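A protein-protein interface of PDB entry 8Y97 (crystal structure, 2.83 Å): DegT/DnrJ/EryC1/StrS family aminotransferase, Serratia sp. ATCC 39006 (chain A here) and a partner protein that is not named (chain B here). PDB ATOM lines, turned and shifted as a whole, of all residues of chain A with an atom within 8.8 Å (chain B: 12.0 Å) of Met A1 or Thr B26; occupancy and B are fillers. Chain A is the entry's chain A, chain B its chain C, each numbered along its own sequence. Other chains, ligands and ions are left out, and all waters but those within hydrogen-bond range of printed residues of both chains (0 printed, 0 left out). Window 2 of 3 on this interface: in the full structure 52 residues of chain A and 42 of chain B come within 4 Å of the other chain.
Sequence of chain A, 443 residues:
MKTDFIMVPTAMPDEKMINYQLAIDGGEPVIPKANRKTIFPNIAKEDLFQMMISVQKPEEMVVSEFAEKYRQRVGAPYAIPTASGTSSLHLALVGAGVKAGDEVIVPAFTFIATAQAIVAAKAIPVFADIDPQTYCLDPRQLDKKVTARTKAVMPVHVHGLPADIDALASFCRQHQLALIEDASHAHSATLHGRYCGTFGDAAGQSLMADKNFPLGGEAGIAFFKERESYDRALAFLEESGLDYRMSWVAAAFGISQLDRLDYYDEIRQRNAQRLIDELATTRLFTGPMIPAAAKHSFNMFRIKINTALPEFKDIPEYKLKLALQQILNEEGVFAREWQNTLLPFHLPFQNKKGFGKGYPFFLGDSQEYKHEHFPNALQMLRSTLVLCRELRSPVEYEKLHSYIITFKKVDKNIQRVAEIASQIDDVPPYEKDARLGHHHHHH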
ATOM      1  N   MET A   1      26.260  29.034  38.494  1.00  0.00           N
ATOM      2  CA  MET A   1      26.055  29.225  37.032  1.00  0.00           C
ATOM      3  C   MET A   1      27.127  30.168  36.491  1.00  0.00           C
ATOM      4  O   MET A   1      27.373  31.220  37.074  1.00  0.00           O
ATOM      5  CB  MET A   1      24.669  29.811  36.742  1.00  0.00           C
ATOM      6  CG  MET A   1      24.334  29.889  35.264  1.00  0.00           C
ATOM      7  SD  MET A   1      22.745  30.672  34.928  1.00  0.00           S
ATOM      8  CE  MET A   1      23.087  32.322  35.556  1.00  0.00           C
ATOM      9  N   LYS A   2      27.746  29.784  35.369  1.00  0.00           N
ATOM     10  CA  LYS A   2      28.820  30.563  34.775  1.00  0.00           C
ATOM     11  C   LYS A   2      28.218  31.478  33.712  1.00  0.00           C
ATOM     12  O   LYS A   2      27.728  31.002  32.689  1.00  0.00           O
ATOM     13  CB  LYS A   2      29.871  29.604  34.198  1.00  0.00           C
ATOM     14  CG  LYS A   2      31.342  29.956  34.429  1.00  0.00           C
ATOM     15  CD  LYS A   2      31.878  31.295  33.928  1.00  0.00           C
ATOM     16  CE  LYS A   2      31.866  31.445  32.438  1.00  0.00           C
ATOM     17  NZ  LYS A   2      32.727  30.465  31.769  1.00  0.00           N
ATOM     18  N   THR A   3      28.227  32.789  33.983  1.00  0.00           N
ATOM     19  CA  THR A   3      27.577  33.773  33.133  1.00  0.00           C
ATOM     20  C   THR A   3      28.492  34.986  32.975  1.00  0.00           C
ATOM     21  O   THR A   3      29.274  35.302  33.869  1.00  0.00           O
ATOM     22  CB  THR A   3      26.222  34.157  33.730  1.00  0.00           C
ATOM     23  OG1 THR A   3      25.698  35.168  32.875  1.00  0.00           O
ATOM     24  CG2 THR A   3      26.317  34.700  35.145  1.00  0.00           C
ATOM     25  N   ASP A   4      28.357  35.670  31.833  1.00  0.00           N
ATOM     26  CA  ASP A   4      29.134  36.862  31.534  1.00  0.00           C
ATOM     27  C   ASP A   4      28.399  38.113  32.018  1.00  0.00           C
ATOM     28  O   ASP A   4      28.894  39.222  31.845  1.00  0.00           O
ATOM     29  CB  ASP A   4      29.445  36.952  30.047  1.00  0.00           C
ATOM     30  CG  ASP A   4      28.243  36.921  29.113  1.00  0.00           C
ATOM     31  OD1 ASP A   4      27.129  36.627  29.592  1.00  0.00           O
ATOM     32  OD2 ASP A   4      28.422  37.203  27.911  1.00  0.00           O
ATOM     33  N   PHE A   5      27.224  37.934  32.631  1.00  0.00           N
ATOM     34  CA  PHE A   5      26.341  39.047  32.936  1.00  0.00           C
ATOM     35  C   PHE A   5      27.062  40.048  33.836  1.00  0.00           C
ATOM     36  O   PHE A   5      27.619  39.673  34.865  1.00  0.00           O
ATOM     37  CB  PHE A   5      25.051  38.522  33.571  1.00  0.00           C
ATOM     38  CG  PHE A   5      23.995  39.595  33.789  1.00  0.00           C
ATOM     39  CD1 PHE A   5      23.111  39.940  32.772  1.00  0.00           C
ATOM     40  CD2 PHE A   5      23.903  40.269  35.004  1.00  0.00           C
ATOM     41  CE1 PHE A   5      22.156  40.927  32.968  1.00  0.00           C
ATOM     42  CE2 PHE A   5      22.943  41.253  35.195  1.00  0.00           C
ATOM     43  CZ  PHE A   5      22.070  41.576  34.179  1.00  0.00           C
ATOM     44  N   ILE A  39      29.726  43.150  26.610  1.00  0.00           N
ATOM     45  CA  ILE A  39      29.213  41.865  26.170  1.00  0.00           C
ATOM     46  C   ILE A  39      29.147  41.875  24.648  1.00  0.00           C
ATOM     47  O   ILE A  39      28.535  42.763  24.056  1.00  0.00           O
ATOM     48  CB  ILE A  39      27.828  41.581  26.787  1.00  0.00           C
ATOM     49  CG1 ILE A  39      27.851  41.642  28.319  1.00  0.00           C
ATOM     50  CG2 ILE A  39      27.267  40.253  26.278  1.00  0.00           C
ATOM     51  CD1 ILE A  39      28.817  40.666  28.965  1.00  0.00           C
ATOM     52  N   ILE A  43      23.942  37.869  23.378  1.00  0.00           N
ATOM     53  CA  ILE A  43      23.300  36.568  23.480  1.00  0.00           C
ATOM     54  C   ILE A  43      22.040  36.718  24.327  1.00  0.00           C
ATOM     55  O   ILE A  43      22.117  37.017  25.516  1.00  0.00           O
ATOM     56  CB  ILE A  43      24.270  35.514  24.045  1.00  0.00           C
ATOM     57  CG1 ILE A  43      25.563  35.450  23.230  1.00  0.00           C
ATOM     58  CG2 ILE A  43      23.603  34.140  24.130  1.00  0.00           C
ATOM     59  CD1 ILE A  43      26.710  34.762  23.944  1.00  0.00           C
ATOM     60  N   ALA A  44      20.885  36.506  23.689  1.00  0.00           N
ATOM     61  CA  ALA A  44      19.592  36.662  24.330  1.00  0.00           C
ATOM     62  C   ALA A  44      18.880  35.313  24.395  1.00  0.00           C
ATOM     63  O   ALA A  44      19.370  34.319  23.859  1.00  0.00           O
ATOM     64  CB  ALA A  44      18.776  37.685  23.570  1.00  0.00           C
ATOM     65  N   LYS A  45      17.719  35.304  25.060  1.00  0.00           N
ATOM     66  CA  LYS A  45      16.885  34.118  25.191  1.00  0.00           C
ATOM     67  C   LYS A  45      16.558  33.532  23.818  1.00  0.00           C
ATOM     68  O   LYS A  45      16.511  32.314  23.660  1.00  0.00           O
ATOM     69  CB  LYS A  45      15.600  34.471  25.950  1.00  0.00           C
ATOM     70  CG  LYS A  45      14.707  35.519  25.291  1.00  0.00           C
ATOM     71  CD  LYS A  45      13.556  35.984  26.174  1.00  0.00           C
ATOM     72  CE  LYS A  45      12.651  36.943  25.470  1.00  0.00           C
ATOM     73  NZ  LYS A  45      11.437  37.200  26.248  1.00  0.00           N
ATOM     74  N   ASP A  47      18.295  33.296  21.242  1.00  0.00           N
ATOM     75  CA  ASP A  47      19.398  32.543  20.669  1.00  0.00           C
ATOM     76  C   ASP A  47      19.438  31.136  21.266  1.00  0.00           C
ATOM     77  O   ASP A  47      19.727  30.174  20.553  1.00  0.00           O
ATOM     78  CB  ASP A  47      20.703  33.312  20.808  1.00  0.00           C
ATOM     79  CG  ASP A  47      20.692  34.715  20.215  1.00  0.00           C
ATOM     80  OD1 ASP A  47      20.278  34.856  19.046  1.00  0.00           O
ATOM     81  OD2 ASP A  47      21.099  35.657  20.924  1.00  0.00           O
ATOM     82  N   LEU A  48      19.143  31.021  22.569  1.00  0.00           N
ATOM     83  CA  LEU A  48      19.090  29.727  23.234  1.00  0.00           C
ATOM     84  C   LEU A  48      17.917  28.918  22.691  1.00  0.00           C
ATOM     85  O   LEU A  48      18.051  27.722  22.445  1.00  0.00           O
ATOM     86  CB  LEU A  48      18.996  29.862  24.753  1.00  0.00           C
ATOM     87  CG  LEU A  48      20.330  30.058  25.480  1.00  0.00           C
ATOM     88  CD1 LEU A  48      20.887  31.445  25.206  1.00  0.00           C
ATOM     89  CD2 LEU A  48      20.190  29.803  26.972  1.00  0.00           C
ATOM     90  N   PHE A 253      22.692  30.172  15.340  1.00  0.00           N
ATOM     91  CA  PHE A 253      22.927  31.425  16.036  1.00  0.00           C
ATOM     92  C   PHE A 253      22.696  32.595  15.080  1.00  0.00           C
ATOM     93  O   PHE A 253      22.161  33.627  15.480  1.00  0.00           O
ATOM     94  CB  PHE A 253      24.345  31.399  16.611  1.00  0.00           C
ATOM     95  CG  PHE A 253      24.648  32.501  17.613  1.00  0.00           C
ATOM     96  CD1 PHE A 253      24.320  32.353  18.957  1.00  0.00           C
ATOM     97  CD2 PHE A 253      25.270  33.677  17.209  1.00  0.00           C
ATOM     98  CE1 PHE A 253      24.604  33.357  19.868  1.00  0.00           C
ATOM     99  CE2 PHE A 253      25.554  34.676  18.123  1.00  0.00           C
ATOM    100  CZ  PHE A 253      25.222  34.513  19.451  1.00  0.00           C
ATOM    101  N   PHE B  15      18.056  16.893  24.713  1.00  0.00           N
ATOM    102  CA  PHE B  15      18.192  17.666  25.937  1.00  0.00           C
ATOM    103  C   PHE B  15      19.669  17.922  26.226  1.00  0.00           C
ATOM    104  O   PHE B  15      20.059  19.057  26.502  1.00  0.00           O
ATOM    105  CB  PHE B  15      17.516  16.966  27.122  1.00  0.00           C
ATOM    106  CG  PHE B  15      17.715  17.687  28.448  1.00  0.00           C
ATOM    107  CD1 PHE B  15      17.043  18.873  28.727  1.00  0.00           C
ATOM    108  CD2 PHE B  15      18.581  17.180  29.413  1.00  0.00           C
ATOM    109  CE1 PHE B  15      17.233  19.532  29.933  1.00  0.00           C
ATOM    110  CE2 PHE B  15      18.762  17.839  30.621  1.00  0.00           C
ATOM    111  CZ  PHE B  15      18.090  19.012  30.878  1.00  0.00           C
ATOM    112  N   GLN B  16      20.476  16.856  26.167  1.00  0.00           N
ATOM    113  CA  GLN B  16      21.895  16.929  26.481  1.00  0.00           C
ATOM    114  C   GLN B  16      22.599  17.914  25.549  1.00  0.00           C
ATOM    115  O   GLN B  16      23.453  18.680  25.997  1.00  0.00           O
ATOM    116  CB  GLN B  16      22.513  15.531  26.414  1.00  0.00           C
ATOM    117  CG  GLN B  16      22.081  14.612  27.553  1.00  0.00           C
ATOM    118  CD  GLN B  16      22.374  13.149  27.293  1.00  0.00           C
ATOM    119  OE1 GLN B  16      22.876  12.763  26.231  1.00  0.00           O
ATOM    120  NE2 GLN B  16      22.042  12.309  28.263  1.00  0.00           N
ATOM    121  N   VAL B  17      22.233  17.890  24.260  1.00  0.00           N
ATOM    122  CA  VAL B  17      22.789  18.800  23.271  1.00  0.00           C
ATOM    123  C   VAL B  17      22.361  20.227  23.606  1.00  0.00           C
ATOM    124  O   VAL B  17      23.198  21.124  23.677  1.00  0.00           O
ATOM    125  CB  VAL B  17      22.377  18.409  21.839  1.00  0.00           C
ATOM    126  CG1 VAL B  17      22.747  19.477  20.816  1.00  0.00           C
ATOM    127  CG2 VAL B  17      22.972  17.066  21.435  1.00  0.00           C
ATOM    128  N   SER B  18      21.053  20.420  23.806  1.00  0.00           N
ATOM    129  CA  SER B  18      20.498  21.726  24.126  1.00  0.00           C
ATOM    130  C   SER B  18      21.137  22.289  25.394  1.00  0.00           C
ATOM    131  O   SER B  18      21.421  23.484  25.468  1.00  0.00           O
ATOM    132  CB  SER B  18      18.991  21.661  24.265  1.00  0.00           C
ATOM    133  OG  SER B  18      18.374  21.303  23.038  1.00  0.00           O
ATOM    134  N   PHE B  19      21.354  21.421  26.389  1.00  0.00           N
ATOM    135  CA  PHE B  19      21.850  21.850  27.685  1.00  0.00           C
ATOM    136  C   PHE B  19      23.259  22.421  27.535  1.00  0.00           C
ATOM    137  O   PHE B  19      23.573  23.459  28.118  1.00  0.00           O
ATOM    138  CB  PHE B  19      21.827  20.692  28.688  1.00  0.00           C
ATOM    139  CG  PHE B  19      22.315  21.076  30.078  1.00  0.00           C
ATOM    140  CD1 PHE B  19      23.670  21.040  30.392  1.00  0.00           C
ATOM    141  CD2 PHE B  19      21.421  21.492  31.060  1.00  0.00           C
ATOM    142  CE1 PHE B  19      24.115  21.403  31.655  1.00  0.00           C
ATOM    143  CE2 PHE B  19      21.872  21.852  32.322  1.00  0.00           C
ATOM    144  CZ  PHE B  19      23.216  21.807  32.617  1.00  0.00           C
ATOM    145  N   VAL B  20      24.099  21.729  26.755  1.00  0.00           N
ATOM    146  CA  VAL B  20      25.492  22.116  26.615  1.00  0.00           C
ATOM    147  C   VAL B  20      25.579  23.408  25.800  1.00  0.00           C
ATOM    148  O   VAL B  20      26.363  24.294  26.138  1.00  0.00           O
ATOM    149  CB  VAL B  20      26.375  20.975  26.063  1.00  0.00           C
ATOM    150  CG1 VAL B  20      26.068  20.584  24.622  1.00  0.00           C
ATOM    151  CG2 VAL B  20      27.857  21.290  26.218  1.00  0.00           C
ATOM    152  N   LEU B  21      24.752  23.528  24.754  1.00  0.00           N
ATOM    153  CA  LEU B  21      24.702  24.736  23.947  1.00  0.00           C
ATOM    154  C   LEU B  21      24.223  25.913  24.794  1.00  0.00           C
ATOM    155  O   LEU B  21      24.722  27.024  24.646  1.00  0.00           O
ATOM    156  CB  LEU B  21      23.800  24.509  22.736  1.00  0.00           C
ATOM    157  CG  LEU B  21      24.328  23.522  21.689  1.00  0.00           C
ATOM    158  CD1 LEU B  21      23.235  23.146  20.706  1.00  0.00           C
ATOM    159  CD2 LEU B  21      25.524  24.105  20.956  1.00  0.00           C
ATOM    160  N   ALA B  22      23.260  25.658  25.687  1.00  0.00           N
ATOM    161  CA  ALA B  22      22.740  26.685  26.575  1.00  0.00           C
ATOM    162  C   ALA B  22      23.817  27.126  27.567  1.00  0.00           C
ATOM    163  O   ALA B  22      23.970  28.321  27.816  1.00  0.00           O
ATOM    164  CB  ALA B  22      21.506  26.179  27.288  1.00  0.00           C
ATOM    165  N   ARG B  23      24.557  26.155  28.123  1.00  0.00           N
ATOM    166  CA  ARG B  23      25.585  26.430  29.116  1.00  0.00           C
ATOM    167  C   ARG B  23      26.653  27.350  28.529  1.00  0.00           C
ATOM    168  O   ARG B  23      27.008  28.358  29.138  1.00  0.00           O
ATOM    169  CB  ARG B  23      26.234  25.135  29.624  1.00  0.00           C
ATOM    170  CG  ARG B  23      27.293  25.343  30.700  1.00  0.00           C
ATOM    171  CD  ARG B  23      27.870  24.035  31.232  1.00  0.00           C
ATOM    172  NE  ARG B  23      28.499  23.208  30.193  1.00  0.00           N
ATOM    173  CZ  ARG B  23      29.595  23.521  29.508  1.00  0.00           C
ATOM    174  NH1 ARG B  23      30.240  24.650  29.746  1.00  0.00           N
ATOM    175  NH2 ARG B  23      30.051  22.697  28.580  1.00  0.00           N
ATOM    176  N   VAL B  24      27.164  26.988  27.347  1.00  0.00           N
ATOM    177  CA  VAL B  24      28.242  27.731  26.715  1.00  0.00           C
ATOM    178  C   VAL B  24      27.724  29.103  26.286  1.00  0.00           C
ATOM    179  O   VAL B  24      28.428  30.100  26.430  1.00  0.00           O
ATOM    180  CB  VAL B  24      28.851  26.956  25.530  1.00  0.00           C
ATOM    181  CG1 VAL B  24      29.886  27.783  24.775  1.00  0.00           C
ATOM    182  CG2 VAL B  24      29.460  25.636  25.979  1.00  0.00           C
ATOM    183  N   LEU B  25      26.494  29.149  25.761  1.00  0.00           N
ATOM    184  CA  LEU B  25      25.890  30.407  25.350  1.00  0.00           C
ATOM    185  C   LEU B  25      25.703  31.313  26.567  1.00  0.00           C
ATOM    186  O   LEU B  25      25.863  32.529  26.462  1.00  0.00           O
ATOM    187  CB  LEU B  25      24.567  30.166  24.624  1.00  0.00           C
ATOM    188  CG  LEU B  25      24.665  29.643  23.188  1.00  0.00           C
ATOM    189  CD1 LEU B  25      23.290  29.223  22.695  1.00  0.00           C
ATOM    190  CD2 LEU B  25      25.265  30.677  22.259  1.00  0.00           C
ATOM    191  N   THR B  26      25.373  30.714  27.717  1.00  0.00           N
ATOM    192  CA  THR B  26      25.207  31.468  28.950  1.00  0.00           C
ATOM    193  C   THR B  26      26.558  32.023  29.398  1.00  0.00           C
ATOM    194  O   THR B  26      26.618  33.137  29.912  1.00  0.00           O
ATOM    195  CB  THR B  26      24.562  30.594  30.026  1.00  0.00           C
ATOM    196  OG1 THR B  26      23.359  30.100  29.448  1.00  0.00           O
ATOM    197  CG2 THR B  26      24.237  31.373  31.289  1.00  0.00           C
ATOM    198  N   SER B  27      27.633  31.251  29.192  1.00  0.00           N
ATOM    199  CA  SER B  27      28.973  31.674  29.573  1.00  0.00           C
ATOM    200  C   SER B  27      29.402  32.896  28.763  1.00  0.00           C
ATOM    201  O   SER B  27      30.138  33.744  29.264  1.00  0.00           O
ATOM    202  CB  SER B  27      29.971  30.552  29.421  1.00  0.00           C
ATOM    203  OG  SER B  27      30.285  30.312  28.057  1.00  0.00           O
ATOM    204  N   GLY B  28      28.943  32.963  27.507  1.00  0.00           N
ATOM    205  CA  GLY B  28      29.243  34.080  26.626  1.00  0.00           C
ATOM    206  C   GLY B  28      30.590  33.914  25.930  1.00  0.00           C
ATOM    207  O   GLY B  28      31.039  34.831  25.244  1.00  0.00           O
ATOM    208  N   ILE B  29      31.213  32.737  26.102  1.00  0.00           N
ATOM    209  CA  ILE B  29      32.528  32.448  25.554  1.00  0.00           C
ATOM    210  C   ILE B  29      32.354  31.502  24.368  1.00  0.00           C
ATOM    211  O   ILE B  29      32.370  30.285  24.539  1.00  0.00           O
ATOM    212  CB  ILE B  29      33.452  31.846  26.632  1.00  0.00           C
ATOM    213  CG1 ILE B  29      33.379  32.614  27.959  1.00  0.00           C
ATOM    214  CG2 ILE B  29      34.890  31.741  26.120  1.00  0.00           C
ATOM    215  CD1 ILE B  29      33.732  34.088  27.852  1.00  0.00           C
ATOM    216  N   ILE B  30      32.182  32.076  23.171  1.00  0.00           N
ATOM    217  CA  ILE B  30      31.862  31.294  21.987  1.00  0.00           C
ATOM    218  C   ILE B  30      32.879  31.533  20.869  1.00  0.00           C
ATOM    219  O   ILE B  30      32.684  31.026  19.767  1.00  0.00           O
ATOM    220  CB  ILE B  30      30.426  31.592  21.512  1.00  0.00           C
ATOM    221  CG1 ILE B  30      30.238  33.055  21.108  1.00  0.00           C
ATOM    222  CG2 ILE B  30      29.406  31.168  22.569  1.00  0.00           C
ATOM    223  CD1 ILE B  30      29.041  33.289  20.206  1.00  0.00           C
ATOM    224  N   MET B  31      33.958  32.279  21.141  1.00  0.00           N
ATOM    225  CA  MET B  31      35.008  32.493  20.156  1.00  0.00           C
ATOM    226  C   MET B  31      36.164  31.530  20.415  1.00  0.00           C
ATOM    227  O   MET B  31      36.510  31.265  21.563  1.00  0.00           O
ATOM    228  CB  MET B  31      35.579  33.911  20.223  1.00  0.00           C
ATOM    229  CG  MET B  31      34.631  35.003  19.794  1.00  0.00           C
ATOM    230  SD  MET B  31      35.471  36.596  19.851  1.00  0.00           S
ATOM    231  CE  MET B  31      34.071  37.704  20.067  1.00  0.00           C
ATOM    232  N   GLU B  34      39.272  33.550  21.939  1.00  0.00           N
ATOM    233  CA  GLU B  34      38.967  34.348  23.115  1.00  0.00           C
ATOM    234  C   GLU B  34      39.618  33.721  24.346  1.00  0.00           C
ATOM    235  O   GLU B  34      39.740  32.501  24.436  1.00  0.00           O
ATOM    236  CB  GLU B  34      37.444  34.438  23.216  1.00  0.00           C
ATOM    237  CG  GLU B  34      36.913  35.224  24.411  1.00  0.00           C
ATOM    238  CD  GLU B  34      35.397  35.306  24.443  1.00  0.00           C
ATOM    239  OE1 GLU B  34      34.751  34.713  23.554  1.00  0.00           O
ATOM    240  OE2 GLU B  34      34.868  35.973  25.356  1.00  0.00           O
ATOM    241  N   ASN B  36      39.906  32.504  28.200  1.00  0.00           N
ATOM    242  CA  ASN B  36      39.010  31.761  29.076  1.00  0.00           C
ATOM    243  C   ASN B  36      38.139  30.792  28.276  1.00  0.00           C
ATOM    244  O   ASN B  36      37.083  30.378  28.753  1.00  0.00           O
ATOM    245  CB  ASN B  36      38.149  32.671  29.948  1.00  0.00           C
ATOM    246  CG  ASN B  36      38.977  33.618  30.782  1.00  0.00           C
ATOM    247  OD1 ASN B  36      39.812  33.176  31.580  1.00  0.00           O
ATOM    248  ND2 ASN B  36      38.755  34.916  30.628  1.00  0.00           N
ATOM    249  N   GLU B  37      38.590  30.420  27.073  1.00  0.00           N
ATOM    250  CA  GLU B  37      37.934  29.382  26.293  1.00  0.00           C
ATOM    251  C   GLU B  37      38.568  28.042  26.652  1.00  0.00           C
ATOM    252  O   GLU B  37      39.743  27.831  26.375  1.00  0.00           O
ATOM    253  CB  GLU B  37      38.036  29.744  24.810  1.00  0.00           C
ATOM    254  CG  GLU B  37      37.629  28.645  23.830  1.00  0.00           C
ATOM    255  CD  GLU B  37      36.606  27.624  24.304  1.00  0.00           C
ATOM    256  OE1 GLU B  37      35.511  27.903  24.843  1.00  0.00           O
ATOM    257  OE2 GLU B  37      36.994  26.468  24.123  1.00  0.00           O
ATOM    258  N   GLU B  39      36.698  24.869  26.294  1.00  0.00           N
ATOM    259  CA  GLU B  39      35.921  23.768  25.741  1.00  0.00           C
ATOM    260  C   GLU B  39      36.788  22.938  24.796  1.00  0.00           C
ATOM    261  O   GLU B  39      36.720  21.712  24.803  1.00  0.00           O
ATOM    262  CB  GLU B  39      34.668  24.271  25.020  1.00  0.00           C
ATOM    263  CG  GLU B  39      33.687  25.008  25.927  1.00  0.00           C
ATOM    264  CD  GLU B  39      33.102  24.187  27.065  1.00  0.00           C
ATOM    265  OE1 GLU B  39      32.718  23.021  26.824  1.00  0.00           O
ATOM    266  OE2 GLU B  39      33.003  24.727  28.189  1.00  0.00           O
ATOM    267  N   PRO B 195      33.912  26.817  19.459  1.00  0.00           N
ATOM    268  CA  PRO B 195      33.756  26.287  20.815  1.00  0.00           C
ATOM    269  C   PRO B 195      32.440  25.548  21.046  1.00  0.00           C
ATOM    270  O   PRO B 195      32.430  24.487  21.665  1.00  0.00           O
ATOM    271  CB  PRO B 195      33.863  27.549  21.677  1.00  0.00           C
ATOM    272  CG  PRO B 195      34.796  28.440  20.895  1.00  0.00           C
ATOM    273  CD  PRO B 195      34.435  28.191  19.444  1.00  0.00           C
ATOM    274  N   LEU B 196      31.339  26.116  20.542  1.00  0.00           N
ATOM    275  CA  LEU B 196      30.027  25.504  20.683  1.00  0.00           C
ATOM    276  C   LEU B 196      30.056  24.084  20.124  1.00  0.00           C
ATOM    277  O   LEU B 196      29.574  23.159  20.773  1.00  0.00           O
ATOM    278  CB  LEU B 196      28.952  26.349  20.000  1.00  0.00           C
ATOM    279  CG  LEU B 196      28.493  27.601  20.755  1.00  0.00           C
ATOM    280  CD1 LEU B 196      27.634  28.470  19.856  1.00  0.00           C
ATOM    281  CD2 LEU B 196      27.733  27.242  22.021  1.00  0.00           C
ATOM    282  N   ALA B 199      32.211  21.832  22.332  1.00  0.00           N
ATOM    283  CA  ALA B 199      31.574  21.488  23.594  1.00  0.00           C
ATOM    284  C   ALA B 199      30.591  20.336  23.405  1.00  0.00           C
ATOM    285  O   ALA B 199      30.460  19.488  24.287  1.00  0.00           O
ATOM    286  CB  ALA B 199      30.887  22.706  24.171  1.00  0.00           C
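OG1 of Thr A3 sits at hydrogen-bond distance from N of Phe A5 (3.2 Å).
The backbone carbonyl oxygen of Ala B22 lies within hydrogen-bond range of the side-chain hydroxyl of Thr B26, 2.5 Å away.
The backbone carbonyl oxygen of Val B24 lies within hydrogen-bond range of the side-chain hydroxyl of Ser B27 (2.5 Å).
The backbone NH (N) of Ile B29 lies close to the side-chain hydroxyl (OG) of Ser B27 (3.3 Å).
Among the printed residues, pairs that only touch across the chains: Met A1 with Thr B26 (3.99 Å), Lys A2 with Thr B26 (3.6 Å), Lys A2 with Ser B27 (3.4 Å), Thr A3 with Thr B26 (3.4 Å), Asp A4 with Thr B26 (3.5 Å), Asp A4 with Ser B27 (3.4 Å), Asp A4 with Gly B28 (3.5 Å), Ile A43 with Leu B25 (3.5 Å), Ile A43 with Gly B28 (3.8 Å), Leu A48 with Ala B22 (3.9 Å), Leu A48 with Leu B25 (3.9 Å) and Phe A253 with Leu B25 (3.7 Å).
Of the printed residues of chain B, Met A1 touches Thr B26.
Of the printed residues of chain A, Thr B26 touches Met A1 (3.99 Å), Lys A2 (3.6 Å), Thr A3 (3.4 Å) and Asp A4 (3.5 Å).
Thr A3 touches just one residue of chain B: Thr B26.
Ser B27 touches just these residues of chain A: Lys A2 (3.4 Å) and Asp A4 (3.4 Å).
Printed residues of chain B within 4 Å of Ile A43: Leu B25 (3.5 Å) and Gly B28 (3.8 Å).
Printed residues of chain A within 4 Å of Ala B22: Leu A48 (3.9 Å).
Printed residues of chain A within 4 Å of Gly B28: Asp A4 (3.5 Å) and Ile A43 (3.8 Å).
Glu B39 touches none of the printed residues of chain A.
Phe B19 touches none of the printed residues of chain A.
The nearest printed residue of chain B that does not touch Met A1 is Arg B23 (6.9 Å).
The nearest printed residue of chain A that does not touch Gly B28 is Lys A2 (5.7 Å).
Printed residues of chain B that touch a printed residue of chain A: Ala B22, Leu B25, Thr B26, Ser B27 and Gly B28.
Hydrophobic or aromatic side chains of chain B that line the printed part of chain A: Ala B22 and Leu B25.
Among the printed residues, no Asp or Glu carboxylate lies within 4 Å of a Lys or Arg side-chain nitrogen of the other chain.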
